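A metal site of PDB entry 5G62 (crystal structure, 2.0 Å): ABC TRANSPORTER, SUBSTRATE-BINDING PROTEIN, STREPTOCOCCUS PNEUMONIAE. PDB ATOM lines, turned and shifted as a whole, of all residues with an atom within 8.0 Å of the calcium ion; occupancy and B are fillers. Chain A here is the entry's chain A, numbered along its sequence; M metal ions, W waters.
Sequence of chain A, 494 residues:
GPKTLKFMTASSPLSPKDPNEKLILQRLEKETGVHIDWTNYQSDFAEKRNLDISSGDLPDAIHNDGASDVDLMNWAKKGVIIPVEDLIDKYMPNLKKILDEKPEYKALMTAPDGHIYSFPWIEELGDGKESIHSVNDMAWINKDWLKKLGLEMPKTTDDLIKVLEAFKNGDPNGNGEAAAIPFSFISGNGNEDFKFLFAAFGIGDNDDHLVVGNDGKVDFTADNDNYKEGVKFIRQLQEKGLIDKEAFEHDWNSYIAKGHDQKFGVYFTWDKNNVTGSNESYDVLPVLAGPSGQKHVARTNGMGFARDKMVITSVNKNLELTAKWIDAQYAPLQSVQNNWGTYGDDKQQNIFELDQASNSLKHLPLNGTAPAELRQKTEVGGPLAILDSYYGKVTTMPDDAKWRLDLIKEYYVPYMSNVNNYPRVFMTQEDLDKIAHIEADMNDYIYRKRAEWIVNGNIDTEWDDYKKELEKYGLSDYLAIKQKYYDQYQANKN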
ATOM      1  N   ILE A 203      24.603 -27.931 -11.043  1.00  0.00           N
ATOM      2  CA  ILE A 203      24.621 -26.704 -10.217  1.00  0.00           C
ATOM      3  C   ILE A 203      25.428 -25.587 -10.889  1.00  0.00           C
ATOM      4  O   ILE A 203      24.899 -24.508 -11.115  1.00  0.00           O
ATOM      5  CB  ILE A 203      25.138 -26.953  -8.784  1.00  0.00           C
ATOM      6  CG1 ILE A 203      24.294 -28.017  -8.077  1.00  0.00           C
ATOM      7  CG2 ILE A 203      25.220 -25.584  -7.932  1.00  0.00           C
ATOM      8  CD1 ILE A 203      24.681 -28.248  -6.551  1.00  0.00           C
ATOM      9  N   HIS A 209      29.446 -16.681  -7.392  1.00  0.00           N
ATOM     10  CA  HIS A 209      29.545 -17.994  -6.749  1.00  0.00           C
ATOM     11  C   HIS A 209      28.315 -18.268  -5.880  1.00  0.00           C
ATOM     12  O   HIS A 209      28.417 -18.830  -4.786  1.00  0.00           O
ATOM     13  CB  HIS A 209      30.839 -18.141  -5.942  1.00  0.00           C
ATOM     14  CG  HIS A 209      32.076 -17.766  -6.708  1.00  0.00           C
ATOM     15  ND1 HIS A 209      32.419 -18.368  -7.907  1.00  0.00           N
ATOM     16  CD2 HIS A 209      33.023 -16.836  -6.455  1.00  0.00           C
ATOM     17  CE1 HIS A 209      33.514 -17.792  -8.373  1.00  0.00           C
ATOM     18  NE2 HIS A 209      33.899 -16.860  -7.515  1.00  0.00           N
ATOM     19  N   LEU A 210      27.145 -17.878  -6.363  1.00  0.00           N
ATOM     20  CA  LEU A 210      25.939 -17.881  -5.560  1.00  0.00           C
ATOM     21  C   LEU A 210      24.713 -18.134  -6.432  1.00  0.00           C
ATOM     22  O   LEU A 210      24.396 -17.313  -7.306  1.00  0.00           O
ATOM     23  CB  LEU A 210      25.781 -16.551  -4.828  1.00  0.00           C
ATOM     24  CG  LEU A 210      26.060 -16.306  -3.362  1.00  0.00           C
ATOM     25  CD1 LEU A 210      25.165 -15.110  -2.900  1.00  0.00           C
ATOM     26  CD2 LEU A 210      25.842 -17.529  -2.511  1.00  0.00           C
ATOM     27  N   VAL A 211      24.028 -19.235  -6.173  1.00  0.00           N
ATOM     28  CA  VAL A 211      22.768 -19.567  -6.847  1.00  0.00           C
ATOM     29  C   VAL A 211      21.701 -19.810  -5.774  1.00  0.00           C
ATOM     30  O   VAL A 211      22.005 -19.860  -4.582  1.00  0.00           O
ATOM     31  CB  VAL A 211      22.922 -20.764  -7.805  1.00  0.00           C
ATOM     32  CG1 VAL A 211      24.066 -20.531  -8.833  1.00  0.00           C
ATOM     33  CG2 VAL A 211      23.204 -22.077  -7.029  1.00  0.00           C
ATOM     34  N   VAL A 218      19.988 -20.578  -0.385  1.00  0.00           N
ATOM     35  CA  VAL A 218      21.113 -19.976  -1.089  1.00  0.00           C
ATOM     36  C   VAL A 218      22.314 -20.902  -1.008  1.00  0.00           C
ATOM     37  O   VAL A 218      22.628 -21.433   0.057  1.00  0.00           O
ATOM     38  CB  VAL A 218      21.437 -18.606  -0.470  1.00  0.00           C
ATOM     39  CG1 VAL A 218      22.685 -18.011  -1.071  1.00  0.00           C
ATOM     40  CG2 VAL A 218      20.234 -17.623  -0.647  1.00  0.00           C
ATOM     41  N   ASP A 219      22.980 -21.102  -2.135  1.00  0.00           N
ATOM     42  CA  ASP A 219      24.050 -22.081  -2.282  1.00  0.00           C
ATOM     43  C   ASP A 219      25.308 -21.376  -2.759  1.00  0.00           C
ATOM     44  O   ASP A 219      25.350 -20.872  -3.888  1.00  0.00           O
ATOM     45  CB  ASP A 219      23.627 -23.189  -3.262  1.00  0.00           C
ATOM     46  CG  ASP A 219      24.726 -24.265  -3.484  1.00  0.00           C
ATOM     47  OD1 ASP A 219      25.645 -24.272  -2.683  1.00  0.00           O
ATOM     48  OD2 ASP A 219      24.657 -25.089  -4.424  1.00  0.00           O
ATOM     49  N   PHE A 220      26.336 -21.349  -1.915  1.00  0.00           N
ATOM     50  CA  PHE A 220      27.669 -20.942  -2.354  1.00  0.00           C
ATOM     51  C   PHE A 220      28.269 -22.048  -3.228  1.00  0.00           C
ATOM     52  O   PHE A 220      28.430 -23.179  -2.783  1.00  0.00           O
ATOM     53  CB  PHE A 220      28.583 -20.662  -1.146  1.00  0.00           C
ATOM     54  CG  PHE A 220      29.994 -20.299  -1.497  1.00  0.00           C
ATOM     55  CD1 PHE A 220      30.308 -19.046  -1.957  1.00  0.00           C
ATOM     56  CD2 PHE A 220      31.017 -21.239  -1.368  1.00  0.00           C
ATOM     57  CE1 PHE A 220      31.597 -18.713  -2.248  1.00  0.00           C
ATOM     58  CE2 PHE A 220      32.333 -20.920  -1.681  1.00  0.00           C
ATOM     59  CZ  PHE A 220      32.609 -19.659  -2.126  1.00  0.00           C
ATOM     60  N   THR A 221      28.557 -21.721  -4.482  1.00  0.00           N
ATOM     61  CA  THR A 221      28.852 -22.774  -5.475  1.00  0.00           C
ATOM     62  C   THR A 221      30.277 -23.335  -5.379  1.00  0.00           C
ATOM     63  O   THR A 221      30.523 -24.437  -5.869  1.00  0.00           O
ATOM     64  CB  THR A 221      28.648 -22.227  -6.884  1.00  0.00           C
ATOM     65  OG1 THR A 221      29.465 -21.063  -7.055  1.00  0.00           O
ATOM     66  CG2 THR A 221      27.156 -21.879  -7.176  1.00  0.00           C
ATOM     67  N   ALA A 222      31.222 -22.576  -4.855  1.00  0.00           N
ATOM     68  CA  ALA A 222      32.615 -22.943  -5.007  1.00  0.00           C
ATOM     69  C   ALA A 222      33.110 -23.847  -3.868  1.00  0.00           C
ATOM     70  O   ALA A 222      34.309 -24.102  -3.785  1.00  0.00           O
ATOM     71  CB  ALA A 222      33.465 -21.696  -5.139  1.00  0.00           C
ATOM     72  N   ASP A 223      32.232 -24.344  -3.005  1.00  0.00           N
ATOM     73  CA  ASP A 223      32.583 -25.476  -2.151  1.00  0.00           C
ATOM     74  C   ASP A 223      31.810 -26.756  -2.499  1.00  0.00           C
ATOM     75  O   ASP A 223      31.777 -27.685  -1.691  1.00  0.00           O
ATOM     76  CB  ASP A 223      32.405 -25.103  -0.659  1.00  0.00           C
ATOM     77  CG  ASP A 223      30.971 -24.839  -0.275  1.00  0.00           C
ATOM     78  OD1 ASP A 223      30.154 -24.816  -1.181  1.00  0.00           O
ATOM     79  OD2 ASP A 223      30.703 -24.624   0.932  1.00  0.00           O
ATOM     80  N   ASN A 224      31.194 -26.821  -3.675  1.00  0.00           N
ATOM     81  CA  ASN A 224      30.368 -27.969  -4.016  1.00  0.00           C
ATOM     82  C   ASN A 224      31.220 -29.089  -4.612  1.00  0.00           C
ATOM     83  O   ASN A 224      32.167 -28.818  -5.350  1.00  0.00           O
ATOM     84  CB  ASN A 224      29.287 -27.582  -5.026  1.00  0.00           C
ATOM     85  CG  ASN A 224      28.178 -26.723  -4.412  1.00  0.00           C
ATOM     86  OD1 ASN A 224      28.046 -26.650  -3.213  1.00  0.00           O
ATOM     87  ND2 ASN A 224      27.351 -26.131  -5.256  1.00  0.00           N
ATOM     88  N   ASP A 225      30.879 -30.335  -4.303  1.00  0.00           N
ATOM     89  CA  ASP A 225      31.491 -31.472  -5.010  1.00  0.00           C
ATOM     90  C   ASP A 225      31.367 -31.272  -6.521  1.00  0.00           C
ATOM     91  O   ASP A 225      32.279 -31.631  -7.280  1.00  0.00           O
ATOM     92  CB  ASP A 225      30.841 -32.791  -4.601  1.00  0.00           C
ATOM     93  CG  ASP A 225      31.205 -33.237  -3.192  1.00  0.00           C
ATOM     94  OD1 ASP A 225      32.105 -32.663  -2.562  1.00  0.00           O
ATOM     95  OD2 ASP A 225      30.597 -34.206  -2.728  1.00  0.00           O
ATOM     96  N   ASN A 226      30.260 -30.669  -6.977  1.00  0.00           N
ATOM     97  CA  ASN A 226      30.051 -30.425  -8.391  1.00  0.00           C
ATOM     98  C   ASN A 226      31.119 -29.469  -8.958  1.00  0.00           C
ATOM     99  O   ASN A 226      31.567 -29.637 -10.086  1.00  0.00           O
ATOM    100  CB  ASN A 226      28.657 -29.845  -8.638  1.00  0.00           C
ATOM    101  CG  ASN A 226      27.560 -30.582  -7.847  1.00  0.00           C
ATOM    102  OD1 ASN A 226      27.454 -30.448  -6.638  1.00  0.00           O
ATOM    103  ND2 ASN A 226      26.749 -31.345  -8.563  1.00  0.00           N
ATOM    104  N   TYR A 227      31.461 -28.444  -8.202  1.00  0.00           N
ATOM    105  CA  TYR A 227      32.496 -27.498  -8.607  1.00  0.00           C
ATOM    106  C   TYR A 227      33.865 -28.183  -8.649  1.00  0.00           C
ATOM    107  O   TYR A 227      34.637 -27.976  -9.585  1.00  0.00           O
ATOM    108  CB  TYR A 227      32.475 -26.323  -7.615  1.00  0.00           C
ATOM    109  CG  TYR A 227      33.459 -25.217  -7.862  1.00  0.00           C
ATOM    110  CD1 TYR A 227      34.782 -25.295  -7.378  1.00  0.00           C
ATOM    111  CD2 TYR A 227      33.071 -24.038  -8.498  1.00  0.00           C
ATOM    112  CE1 TYR A 227      35.662 -24.280  -7.562  1.00  0.00           C
ATOM    113  CE2 TYR A 227      33.934 -23.008  -8.697  1.00  0.00           C
ATOM    114  CZ  TYR A 227      35.225 -23.125  -8.233  1.00  0.00           C
ATOM    115  OH  TYR A 227      36.075 -22.096  -8.405  1.00  0.00           O
ATOM    116  N   LYS A 467      38.309 -25.991   1.742  1.00  0.00           N
ATOM    117  CA  LYS A 467      37.033 -25.671   2.364  1.00  0.00           C
ATOM    118  C   LYS A 467      37.223 -25.189   3.808  1.00  0.00           C
ATOM    119  O   LYS A 467      36.544 -24.272   4.244  1.00  0.00           O
ATOM    120  CB  LYS A 467      36.078 -26.852   2.289  1.00  0.00           C
ATOM    121  CG  LYS A 467      35.563 -27.078   0.883  1.00  0.00           C
ATOM    122  CD  LYS A 467      34.460 -28.129   0.832  1.00  0.00           C
ATOM    123  CE  LYS A 467      34.940 -29.455   1.370  1.00  0.00           C
ATOM    124  NZ  LYS A 467      33.866 -30.463   1.468  1.00  0.00           N
ATOM    125  N   LEU A 475      33.059 -18.046   5.578  1.00  0.00           N
ATOM    126  CA  LEU A 475      32.048 -18.477   4.603  1.00  0.00           C
ATOM    127  C   LEU A 475      30.677 -18.715   5.247  1.00  0.00           C
ATOM    128  O   LEU A 475      29.644 -18.359   4.658  1.00  0.00           O
ATOM    129  CB  LEU A 475      32.488 -19.756   3.890  1.00  0.00           C
ATOM    130  CG  LEU A 475      31.457 -20.375   2.947  1.00  0.00           C
ATOM    131  CD1 LEU A 475      31.141 -19.423   1.823  1.00  0.00           C
ATOM    132  CD2 LEU A 475      31.977 -21.735   2.385  1.00  0.00           C
ATOM    133  N   LEU A 479      27.353 -16.750   4.082  1.00  0.00           N
ATOM    134  CA  LEU A 479      26.161 -17.418   3.589  1.00  0.00           C
ATOM    135  C   LEU A 479      24.920 -17.065   4.422  1.00  0.00           C
ATOM    136  O   LEU A 479      23.830 -16.840   3.878  1.00  0.00           O
ATOM    137  CB  LEU A 479      26.382 -18.923   3.575  1.00  0.00           C
ATOM    138  CG  LEU A 479      25.495 -19.756   2.643  1.00  0.00           C
ATOM    139  CD1 LEU A 479      25.494 -19.216   1.241  1.00  0.00           C
ATOM    140  CD2 LEU A 479      25.977 -21.212   2.656  1.00  0.00           C
HETATM  141 CA    CA M   1      27.680 -25.022  -1.524  1.00  0.00          CA
HETATM  142  O   HOH W   1      26.764 -23.564   0.296  1.00  0.00           O
HETATM  143  O   HOH W   2      25.785 -26.718  -0.828  1.00  0.00           O
HETATM  144  O   HOH W   3      28.004 -26.665   0.582  1.00  0.00           O
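The backbone carbonyl oxygen of Val 211 is in hydrogen-bond range of the backbone NH of Asp 219, 2.9 Å away.
Within 4 Å of the calcium ion: Asp 219, Phe 220, Asp 223 and Asn 224.
The calcium ion is bound by O of Phe 220 (2.4 Å), OD1 of Asn 224 (2.4 Å), OD1 of Asp 219 (2.5 Å), OD1 of Asp 223 (2.5 Å), water W1 (2.5 Å), water W2 (2.6 Å) and water W3 (2.7 Å).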
